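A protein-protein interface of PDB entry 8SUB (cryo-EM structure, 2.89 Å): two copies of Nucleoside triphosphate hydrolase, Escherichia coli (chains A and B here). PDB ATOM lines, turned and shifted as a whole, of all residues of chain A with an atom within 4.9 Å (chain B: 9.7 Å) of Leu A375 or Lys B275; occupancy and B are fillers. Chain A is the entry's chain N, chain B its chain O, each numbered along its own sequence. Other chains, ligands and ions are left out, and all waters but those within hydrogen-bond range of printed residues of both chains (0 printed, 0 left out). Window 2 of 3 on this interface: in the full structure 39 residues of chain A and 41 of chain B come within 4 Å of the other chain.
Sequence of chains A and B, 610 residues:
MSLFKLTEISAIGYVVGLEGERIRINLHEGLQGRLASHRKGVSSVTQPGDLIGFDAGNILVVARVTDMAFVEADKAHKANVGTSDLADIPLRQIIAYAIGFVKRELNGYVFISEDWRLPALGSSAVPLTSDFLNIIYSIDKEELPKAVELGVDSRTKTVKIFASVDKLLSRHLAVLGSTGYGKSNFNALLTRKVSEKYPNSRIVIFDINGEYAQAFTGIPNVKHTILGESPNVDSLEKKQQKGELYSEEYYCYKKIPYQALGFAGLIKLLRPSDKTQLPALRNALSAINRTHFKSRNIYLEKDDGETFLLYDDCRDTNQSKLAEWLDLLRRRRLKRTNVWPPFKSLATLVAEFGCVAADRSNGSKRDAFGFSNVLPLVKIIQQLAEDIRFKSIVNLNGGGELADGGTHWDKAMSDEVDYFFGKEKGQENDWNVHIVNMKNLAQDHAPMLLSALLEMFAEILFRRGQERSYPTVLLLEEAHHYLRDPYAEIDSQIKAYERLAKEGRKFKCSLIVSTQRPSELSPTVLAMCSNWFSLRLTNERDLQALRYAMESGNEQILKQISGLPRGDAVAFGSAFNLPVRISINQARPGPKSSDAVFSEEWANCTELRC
The side-chain amide oxygen (OE1) of Gln B277 lies close to the backbone NH (N) of Asp B274, 3.5 Å away.
Of chain B, only Asp B274 and Lys B275 come within 4 Å of Leu A375. Lys B275 touches four residues of chain A. No residue of chain B comes within 4 Å of Val A374. No residue of chain B comes within 4 Å of Pro A376. No residue of chain B comes within 4 Å of Val A378. Of the printed residues of chain A, Leu B278 touches Lys A379 (3.9 Å). Printed residues of chain B within 4 Å of Phe A371: Lys B275. Arg B282 touches none of the printed residues of chain A. The nearest residue of chain A that does not touch Lys B275 is Phe A369 (4.1 Å).
Among the printed residues, pairs that only touch across the chains: Ser A372 with Lys B275, Phe A371 with Lys B275, Leu A375 with Asp B274, Leu A375 with Lys B275, Ala A368 with Lys B275 and Lys A379 with Leu B278.
Positions printed for both chains: 369, 372, 373, 374, 375, 376 and 377. Of the 6 pairs that touch across the chains among the printed residues, none has its exchanged pair printed and touching as well.
Of the 22 printed residues of chain B, 3 touch a printed residue of chain A. Printed residues of chain B that touch a printed residue of chain A: Asp B274, Lys B275 and Leu B278. Hydrophobic or aromatic side chains of chain A within 4 Å of the printed part of chain B: Phe A371 and Leu A375.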
ATOM      1  N   ALA A 368     -10.623  27.307  18.754  1.00  0.00           N
ATOM      2  CA  ALA A 368     -11.175  26.258  17.908  1.00  0.00           C
ATOM      3  C   ALA A 368     -10.263  25.913  16.740  1.00  0.00           C
ATOM      4  O   ALA A 368     -10.509  24.914  16.055  1.00  0.00           O
ATOM      5  CB  ALA A 368     -12.552  26.669  17.379  1.00  0.00           C
ATOM      6  N   PHE A 369      -9.229  26.717  16.491  1.00  0.00           N
ATOM      7  CA  PHE A 369      -8.208  26.380  15.507  1.00  0.00           C
ATOM      8  C   PHE A 369      -7.184  25.387  16.037  1.00  0.00           C
ATOM      9  O   PHE A 369      -6.440  24.805  15.241  1.00  0.00           O
ATOM     10  CB  PHE A 369      -7.489  27.646  15.033  1.00  0.00           C
ATOM     11  CG  PHE A 369      -8.166  28.337  13.888  1.00  0.00           C
ATOM     12  CD1 PHE A 369      -8.140  27.785  12.616  1.00  0.00           C
ATOM     13  CD2 PHE A 369      -8.832  29.536  14.080  1.00  0.00           C
ATOM     14  CE1 PHE A 369      -8.762  28.419  11.557  1.00  0.00           C
ATOM     15  CE2 PHE A 369      -9.458  30.175  13.025  1.00  0.00           C
ATOM     16  CZ  PHE A 369      -9.422  29.616  11.762  1.00  0.00           C
ATOM     17  N   PHE A 371      -8.118  22.833  18.367  1.00  0.00           N
ATOM     18  CA  PHE A 371      -8.807  21.555  18.510  1.00  0.00           C
ATOM     19  C   PHE A 371      -8.750  20.754  17.217  1.00  0.00           C
ATOM     20  O   PHE A 371      -8.728  19.519  17.244  1.00  0.00           O
ATOM     21  CB  PHE A 371     -10.257  21.789  18.928  1.00  0.00           C
ATOM     22  CG  PHE A 371     -10.928  20.576  19.502  1.00  0.00           C
ATOM     23  CD1 PHE A 371     -10.928  20.353  20.867  1.00  0.00           C
ATOM     24  CD2 PHE A 371     -11.559  19.658  18.680  1.00  0.00           C
ATOM     25  CE1 PHE A 371     -11.545  19.243  21.403  1.00  0.00           C
ATOM     26  CE2 PHE A 371     -12.175  18.542  19.210  1.00  0.00           C
ATOM     27  CZ  PHE A 371     -12.168  18.335  20.574  1.00  0.00           C
ATOM     28  N   SER A 372      -8.723  21.442  16.075  1.00  0.00           N
ATOM     29  CA  SER A 372      -8.714  20.753  14.789  1.00  0.00           C
ATOM     30  C   SER A 372      -7.453  19.924  14.612  1.00  0.00           C
ATOM     31  O   SER A 372      -7.474  18.882  13.947  1.00  0.00           O
ATOM     32  CB  SER A 372      -8.843  21.764  13.653  1.00  0.00           C
ATOM     33  OG  SER A 372     -10.161  22.270  13.572  1.00  0.00           O
ATOM     34  N   ASN A 373      -6.342  20.368  15.198  1.00  0.00           N
ATOM     35  CA  ASN A 373      -5.070  19.692  14.983  1.00  0.00           C
ATOM     36  C   ASN A 373      -4.952  18.390  15.765  1.00  0.00           C
ATOM     37  O   ASN A 373      -3.994  17.641  15.549  1.00  0.00           O
ATOM     38  CB  ASN A 373      -3.914  20.622  15.354  1.00  0.00           C
ATOM     39  CG  ASN A 373      -3.855  21.855  14.474  1.00  0.00           C
ATOM     40  OD1 ASN A 373      -3.927  21.761  13.250  1.00  0.00           O
ATOM     41  ND2 ASN A 373      -3.719  23.019  15.097  1.00  0.00           N
ATOM     42  N   VAL A 374      -5.888  18.102  16.669  1.00  0.00           N
ATOM     43  CA  VAL A 374      -5.737  16.964  17.568  1.00  0.00           C
ATOM     44  C   VAL A 374      -7.034  16.162  17.627  1.00  0.00           C
ATOM     45  O   VAL A 374      -7.217  15.308  18.503  1.00  0.00           O
ATOM     46  CB  VAL A 374      -5.304  17.453  18.964  1.00  0.00           C
ATOM     47  CG1 VAL A 374      -6.439  18.186  19.663  1.00  0.00           C
ATOM     48  CG2 VAL A 374      -4.728  16.327  19.801  1.00  0.00           C
ATOM     49  N   LEU A 375      -7.941  16.414  16.690  1.00  0.00           N
ATOM     50  CA  LEU A 375      -9.260  15.788  16.709  1.00  0.00           C
ATOM     51  C   LEU A 375      -9.241  14.300  16.349  1.00  0.00           C
ATOM     52  O   LEU A 375      -9.944  13.514  17.003  1.00  0.00           O
ATOM     53  CB  LEU A 375     -10.214  16.548  15.782  1.00  0.00           C
ATOM     54  CG  LEU A 375     -11.699  16.189  15.860  1.00  0.00           C
ATOM     55  CD1 LEU A 375     -12.536  17.449  15.831  1.00  0.00           C
ATOM     56  CD2 LEU A 375     -12.097  15.272  14.718  1.00  0.00           C
ATOM     57  N   PRO A 376      -8.499  13.862  15.322  1.00  0.00           N
ATOM     58  CA  PRO A 376      -8.497  12.423  15.011  1.00  0.00           C
ATOM     59  C   PRO A 376      -8.043  11.546  16.166  1.00  0.00           C
ATOM     60  O   PRO A 376      -8.555  10.430  16.320  1.00  0.00           O
ATOM     61  CB  PRO A 376      -7.536  12.324  13.819  1.00  0.00           C
ATOM     62  CG  PRO A 376      -7.599  13.645  13.184  1.00  0.00           C
ATOM     63  CD  PRO A 376      -7.764  14.627  14.298  1.00  0.00           C
ATOM     64  N   LEU A 377      -7.100  12.015  16.986  1.00  0.00           N
ATOM     65  CA  LEU A 377      -6.622  11.202  18.098  1.00  0.00           C
ATOM     66  C   LEU A 377      -7.732  10.930  19.106  1.00  0.00           C
ATOM     67  O   LEU A 377      -7.951   9.778  19.502  1.00  0.00           O
ATOM     68  CB  LEU A 377      -5.439  11.887  18.779  1.00  0.00           C
ATOM     69  CG  LEU A 377      -4.712  11.065  19.845  1.00  0.00           C
ATOM     70  CD1 LEU A 377      -4.168   9.783  19.243  1.00  0.00           C
ATOM     71  CD2 LEU A 377      -3.602  11.875  20.490  1.00  0.00           C
ATOM     72  N   VAL A 378      -8.443  11.974  19.537  1.00  0.00           N
ATOM     73  CA  VAL A 378      -9.528  11.756  20.487  1.00  0.00           C
ATOM     74  C   VAL A 378     -10.650  10.967  19.832  1.00  0.00           C
ATOM     75  O   VAL A 378     -11.318  10.165  20.495  1.00  0.00           O
ATOM     76  CB  VAL A 378     -10.028  13.091  21.077  1.00  0.00           C
ATOM     77  CG1 VAL A 378      -8.885  13.832  21.744  1.00  0.00           C
ATOM     78  CG2 VAL A 378     -10.673  13.954  20.014  1.00  0.00           C
ATOM     79  N   LYS A 379     -10.862  11.154  18.526  1.00  0.00           N
ATOM     80  CA  LYS A 379     -11.870  10.367  17.823  1.00  0.00           C
ATOM     81  C   LYS A 379     -11.568   8.877  17.916  1.00  0.00           C
ATOM     82  O   LYS A 379     -12.434   8.079  18.292  1.00  0.00           O
ATOM     83  CB  LYS A 379     -11.949  10.807  16.362  1.00  0.00           C
ATOM     84  CG  LYS A 379     -13.255  10.453  15.679  1.00  0.00           C
ATOM     85  CD  LYS A 379     -13.074  10.362  14.173  1.00  0.00           C
ATOM     86  CE  LYS A 379     -14.408  10.194  13.470  1.00  0.00           C
ATOM     87  NZ  LYS A 379     -14.247   9.589  12.121  1.00  0.00           N
ATOM     88  N   ILE B 267     -22.688   7.957  12.672  1.00  0.00           N
ATOM     89  CA  ILE B 267     -21.463   8.759  12.696  1.00  0.00           C
ATOM     90  C   ILE B 267     -20.633   8.507  11.444  1.00  0.00           C
ATOM     91  O   ILE B 267     -20.087   9.440  10.844  1.00  0.00           O
ATOM     92  CB  ILE B 267     -20.657   8.495  13.981  1.00  0.00           C
ATOM     93  CG1 ILE B 267     -21.257   9.271  15.148  1.00  0.00           C
ATOM     94  CG2 ILE B 267     -19.208   8.895  13.795  1.00  0.00           C
ATOM     95  CD1 ILE B 267     -20.616   8.965  16.466  1.00  0.00           C
ATOM     96  N   ARG B 271     -19.953  11.768   8.724  1.00  0.00           N
ATOM     97  CA  ARG B 271     -18.546  12.071   8.478  1.00  0.00           C
ATOM     98  C   ARG B 271     -18.199  13.521   8.809  1.00  0.00           C
ATOM     99  O   ARG B 271     -18.005  14.336   7.898  1.00  0.00           O
ATOM    100  CB  ARG B 271     -18.182  11.758   7.024  1.00  0.00           C
ATOM    101  CG  ARG B 271     -16.689  11.807   6.741  1.00  0.00           C
ATOM    102  CD  ARG B 271     -16.376  11.652   5.263  1.00  0.00           C
ATOM    103  NE  ARG B 271     -16.890  10.404   4.712  1.00  0.00           N
ATOM    104  CZ  ARG B 271     -17.884  10.327   3.839  1.00  0.00           C
ATOM    105  NH1 ARG B 271     -18.502  11.410   3.397  1.00  0.00           N
ATOM    106  NH2 ARG B 271     -18.265   9.133   3.397  1.00  0.00           N
ATOM    107  N   PRO B 272     -18.137  13.894  10.090  1.00  0.00           N
ATOM    108  CA  PRO B 272     -17.667  15.241  10.456  1.00  0.00           C
ATOM    109  C   PRO B 272     -16.152  15.325  10.336  1.00  0.00           C
ATOM    110  O   PRO B 272     -15.434  14.429  10.782  1.00  0.00           O
ATOM    111  CB  PRO B 272     -18.127  15.396  11.914  1.00  0.00           C
ATOM    112  CG  PRO B 272     -19.007  14.204  12.200  1.00  0.00           C
ATOM    113  CD  PRO B 272     -18.558  13.130  11.272  1.00  0.00           C
ATOM    114  N   SER B 273     -15.665  16.399   9.718  1.00  0.00           N
ATOM    115  CA  SER B 273     -14.232  16.603   9.516  1.00  0.00           C
ATOM    116  C   SER B 273     -13.860  18.069   9.735  1.00  0.00           C
ATOM    117  O   SER B 273     -13.125  18.671   8.951  1.00  0.00           O
ATOM    118  CB  SER B 273     -13.813  16.133   8.124  1.00  0.00           C
ATOM    119  OG  SER B 273     -12.422  16.318   7.919  1.00  0.00           O
ATOM    120  N   ASP B 274     -14.364  18.666  10.813  1.00  0.00           N
ATOM    121  CA  ASP B 274     -14.133  20.084  11.076  1.00  0.00           C
ATOM    122  C   ASP B 274     -13.783  20.261  12.550  1.00  0.00           C
ATOM    123  O   ASP B 274     -13.519  19.291  13.267  1.00  0.00           O
ATOM    124  CB  ASP B 274     -15.348  20.923  10.666  1.00  0.00           C
ATOM    125  CG  ASP B 274     -14.956  22.258  10.068  1.00  0.00           C
ATOM    126  OD1 ASP B 274     -13.891  22.791  10.448  1.00  0.00           O
ATOM    127  OD2 ASP B 274     -15.712  22.774   9.218  1.00  0.00           O
ATOM    128  N   LYS B 275     -13.783  21.516  13.002  1.00  0.00           N
ATOM    129  CA  LYS B 275     -13.247  21.837  14.322  1.00  0.00           C
ATOM    130  C   LYS B 275     -14.136  21.304  15.441  1.00  0.00           C
ATOM    131  O   LYS B 275     -13.677  20.552  16.307  1.00  0.00           O
ATOM    132  CB  LYS B 275     -13.046  23.350  14.457  1.00  0.00           C
ATOM    133  CG  LYS B 275     -14.191  24.211  13.950  1.00  0.00           C
ATOM    134  CD  LYS B 275     -13.694  25.601  13.570  1.00  0.00           C
ATOM    135  CE  LYS B 275     -13.108  25.618  12.169  1.00  0.00           C
ATOM    136  NZ  LYS B 275     -12.588  26.965  11.801  1.00  0.00           N
ATOM    137  N   THR B 276     -15.414  21.683  15.447  1.00  0.00           N
ATOM    138  CA  THR B 276     -16.297  21.371  16.565  1.00  0.00           C
ATOM    139  C   THR B 276     -17.614  20.763  16.083  1.00  0.00           C
ATOM    140  O   THR B 276     -18.696  21.170  16.511  1.00  0.00           O
ATOM    141  CB  THR B 276     -16.539  22.621  17.414  1.00  0.00           C
ATOM    142  OG1 THR B 276     -15.288  23.275  17.650  1.00  0.00           O
ATOM    143  CG2 THR B 276     -17.128  22.254  18.775  1.00  0.00           C
ATOM    144  N   GLN B 277     -17.540  19.793  15.174  1.00  0.00           N
ATOM    145  CA  GLN B 277     -18.742  19.090  14.744  1.00  0.00           C
ATOM    146  C   GLN B 277     -18.983  17.808  15.528  1.00  0.00           C
ATOM    147  O   GLN B 277     -20.141  17.487  15.823  1.00  0.00           O
ATOM    148  CB  GLN B 277     -18.663  18.770  13.250  1.00  0.00           C
ATOM    149  CG  GLN B 277     -18.804  19.978  12.343  1.00  0.00           C
ATOM    150  CD  GLN B 277     -18.402  19.676  10.919  1.00  0.00           C
ATOM    151  OE1 GLN B 277     -17.852  18.617  10.631  1.00  0.00           O
ATOM    152  NE2 GLN B 277     -18.666  20.611  10.019  1.00  0.00           N
ATOM    153  N   LEU B 278     -17.922  17.073  15.871  1.00  0.00           N
ATOM    154  CA  LEU B 278     -18.041  15.791  16.556  1.00  0.00           C
ATOM    155  C   LEU B 278     -18.691  15.904  17.933  1.00  0.00           C
ATOM    156  O   LEU B 278     -19.620  15.141  18.221  1.00  0.00           O
ATOM    157  CB  LEU B 278     -16.673  15.116  16.685  1.00  0.00           C
ATOM    158  CG  LEU B 278     -16.702  13.738  17.354  1.00  0.00           C
ATOM    159  CD1 LEU B 278     -17.518  12.754  16.532  1.00  0.00           C
ATOM    160  CD2 LEU B 278     -15.299  13.210  17.589  1.00  0.00           C
ATOM    161  N   PRO B 279     -18.233  16.792  18.825  1.00  0.00           N
ATOM    162  CA  PRO B 279     -18.879  16.851  20.148  1.00  0.00           C
ATOM    163  C   PRO B 279     -20.333  17.280  20.080  1.00  0.00           C
ATOM    164  O   PRO B 279     -21.173  16.739  20.811  1.00  0.00           O
ATOM    165  CB  PRO B 279     -18.016  17.860  20.916  1.00  0.00           C
ATOM    166  CG  PRO B 279     -17.369  18.678  19.872  1.00  0.00           C
ATOM    167  CD  PRO B 279     -17.129  17.763  18.720  1.00  0.00           C
ATOM    168  N   ALA B 280     -20.656  18.237  19.207  1.00  0.00           N
ATOM    169  CA  ALA B 280     -22.045  18.648  19.048  1.00  0.00           C
ATOM    170  C   ALA B 280     -22.897  17.500  18.526  1.00  0.00           C
ATOM    171  O   ALA B 280     -24.010  17.272  19.014  1.00  0.00           O
ATOM    172  CB  ALA B 280     -22.134  19.852  18.112  1.00  0.00           C
ATOM    173  N   LEU B 281     -22.387  16.760  17.537  1.00  0.00           N
ATOM    174  CA  LEU B 281     -23.135  15.627  17.004  1.00  0.00           C
ATOM    175  C   LEU B 281     -23.343  14.557  18.066  1.00  0.00           C
ATOM    176  O   LEU B 281     -24.436  13.988  18.178  1.00  0.00           O
ATOM    177  CB  LEU B 281     -22.414  15.049  15.787  1.00  0.00           C
ATOM    178  CG  LEU B 281     -23.049  13.820  15.138  1.00  0.00           C
ATOM    179  CD1 LEU B 281     -24.511  14.076  14.826  1.00  0.00           C
ATOM    180  CD2 LEU B 281     -22.298  13.439  13.874  1.00  0.00           C
ATOM    181  N   ARG B 282     -22.308  14.271  18.858  1.00  0.00           N
ATOM    182  CA  ARG B 282     -22.432  13.265  19.908  1.00  0.00           C
ATOM    183  C   ARG B 282     -23.437  13.694  20.968  1.00  0.00           C
ATOM    184  O   ARG B 282     -24.238  12.878  21.440  1.00  0.00           O
ATOM    185  CB  ARG B 282     -21.065  12.995  20.539  1.00  0.00           C
ATOM    186  CG  ARG B 282     -20.056  12.356  19.595  1.00  0.00           C
ATOM    187  CD  ARG B 282     -18.807  11.897  20.329  1.00  0.00           C
ATOM    188  NE  ARG B 282     -18.874  10.491  20.705  1.00  0.00           N
ATOM    189  CZ  ARG B 282     -18.408   9.999  21.843  1.00  0.00           C
ATOM    190  NH1 ARG B 282     -17.821  10.773  22.742  1.00  0.00           N
ATOM    191  NH2 ARG B 282     -18.534   8.697  22.087  1.00  0.00           N
ATOM    192  N   GLY B 354     -24.244  23.797  18.966  1.00  0.00           N
ATOM    193  CA  GLY B 354     -23.034  24.336  18.393  1.00  0.00           C
ATOM    194  C   GLY B 354     -22.866  25.839  18.423  1.00  0.00           C
ATOM    195  O   GLY B 354     -21.863  26.336  17.903  1.00  0.00           O
ATOM    196  N   PHE B 369     -21.113  33.289  15.679  1.00  0.00           N
ATOM    197  CA  PHE B 369     -19.873  32.589  15.362  1.00  0.00           C
ATOM    198  C   PHE B 369     -20.054  31.079  15.445  1.00  0.00           C
ATOM    199  O   PHE B 369     -19.568  30.341  14.580  1.00  0.00           O
ATOM    200  CB  PHE B 369     -18.757  33.048  16.296  1.00  0.00           C
ATOM    201  CG  PHE B 369     -17.394  32.575  15.884  1.00  0.00           C
ATOM    202  CD1 PHE B 369     -17.056  32.486  14.543  1.00  0.00           C
ATOM    203  CD2 PHE B 369     -16.453  32.219  16.832  1.00  0.00           C
ATOM    204  CE1 PHE B 369     -15.807  32.053  14.160  1.00  0.00           C
ATOM    205  CE2 PHE B 369     -15.202  31.783  16.454  1.00  0.00           C
ATOM    206  CZ  PHE B 369     -14.877  31.700  15.116  1.00  0.00           C
ATOM    207  N   GLY B 370     -20.750  30.601  16.478  1.00  0.00           N
ATOM    208  CA  GLY B 370     -21.023  29.176  16.570  1.00  0.00           C
ATOM    209  C   GLY B 370     -21.881  28.677  15.423  1.00  0.00           C
ATOM    210  O   GLY B 370     -21.665  27.579  14.903  1.00  0.00           O
ATOM    211  N   SER B 372     -21.922  29.934  12.407  1.00  0.00           N
ATOM    212  CA  SER B 372     -21.030  29.848  11.255  1.00  0.00           C
ATOM    213  C   SER B 372     -20.153  28.605  11.331  1.00  0.00           C
ATOM    214  O   SER B 372     -19.926  27.932  10.317  1.00  0.00           O
ATOM    215  CB  SER B 372     -20.168  31.104  11.162  1.00  0.00           C
ATOM    216  OG  SER B 372     -19.514  31.357  12.392  1.00  0.00           O
ATOM    217  N   ASN B 373     -19.648  28.288  12.525  1.00  0.00           N
ATOM    218  CA  ASN B 373     -18.787  27.119  12.682  1.00  0.00           C
ATOM    219  C   ASN B 373     -19.535  25.827  12.376  1.00  0.00           C
ATOM    220  O   ASN B 373     -19.002  24.935  11.706  1.00  0.00           O
ATOM    221  CB  ASN B 373     -18.213  27.076  14.099  1.00  0.00           C
ATOM    222  CG  ASN B 373     -16.970  27.931  14.255  1.00  0.00           C
ATOM    223  OD1 ASN B 373     -16.257  28.195  13.286  1.00  0.00           O
ATOM    224  ND2 ASN B 373     -16.704  28.370  15.480  1.00  0.00           N
ATOM    225  N   VAL B 374     -20.779  25.717  12.845  1.00  0.00           N
ATOM    226  CA  VAL B 374     -21.517  24.460  12.800  1.00  0.00           C
ATOM    227  C   VAL B 374     -22.391  24.339  11.553  1.00  0.00           C
ATOM    228  O   VAL B 374     -22.922  23.256  11.275  1.00  0.00           O
ATOM    229  CB  VAL B 374     -22.338  24.313  14.101  1.00  0.00           C
ATOM    230  CG1 VAL B 374     -23.140  23.023  14.149  1.00  0.00           C
ATOM    231  CG2 VAL B 374     -21.414  24.398  15.298  1.00  0.00           C
ATOM    232  N   LEU B 375     -22.498  25.402  10.757  1.00  0.00           N
ATOM    233  CA  LEU B 375     -23.383  25.411   9.591  1.00  0.00           C
ATOM    234  C   LEU B 375     -23.180  24.248   8.619  1.00  0.00           C
ATOM    235  O   LEU B 375     -24.188  23.698   8.149  1.00  0.00           O
ATOM    236  CB  LEU B 375     -23.234  26.756   8.868  1.00  0.00           C
ATOM    237  CG  LEU B 375     -24.377  27.178   7.941  1.00  0.00           C
ATOM    238  CD1 LEU B 375     -25.638  27.473   8.738  1.00  0.00           C
ATOM    239  CD2 LEU B 375     -23.970  28.391   7.125  1.00  0.00           C
ATOM    240  N   PRO B 376     -21.953  23.837   8.258  1.00  0.00           N
ATOM    241  CA  PRO B 376     -21.832  22.775   7.238  1.00  0.00           C
ATOM    242  C   PRO B 376     -22.538  21.474   7.600  1.00  0.00           C
ATOM    243  O   PRO B 376     -23.113  20.825   6.714  1.00  0.00           O
ATOM    244  CB  PRO B 376     -20.313  22.581   7.113  1.00  0.00           C
ATOM    245  CG  PRO B 376     -19.726  23.857   7.579  1.00  0.00           C
ATOM    246  CD  PRO B 376     -20.629  24.352   8.658  1.00  0.00           C
ATOM    247  N   LEU B 377     -22.518  21.073   8.873  1.00  0.00           N
ATOM    248  CA  LEU B 377     -23.185  19.831   9.256  1.00  0.00           C
ATOM    249  C   LEU B 377     -24.697  19.938   9.106  1.00  0.00           C
ATOM    250  O   LEU B 377     -25.352  18.995   8.639  1.00  0.00           O
ATOM    251  CB  LEU B 377     -22.820  19.452  10.690  1.00  0.00           C
ATOM    252  CG  LEU B 377     -23.070  17.979  11.020  1.00  0.00           C
ATOM    253  CD1 LEU B 377     -22.199  17.095  10.142  1.00  0.00           C
ATOM    254  CD2 LEU B 377     -22.821  17.697  12.494  1.00  0.00           C
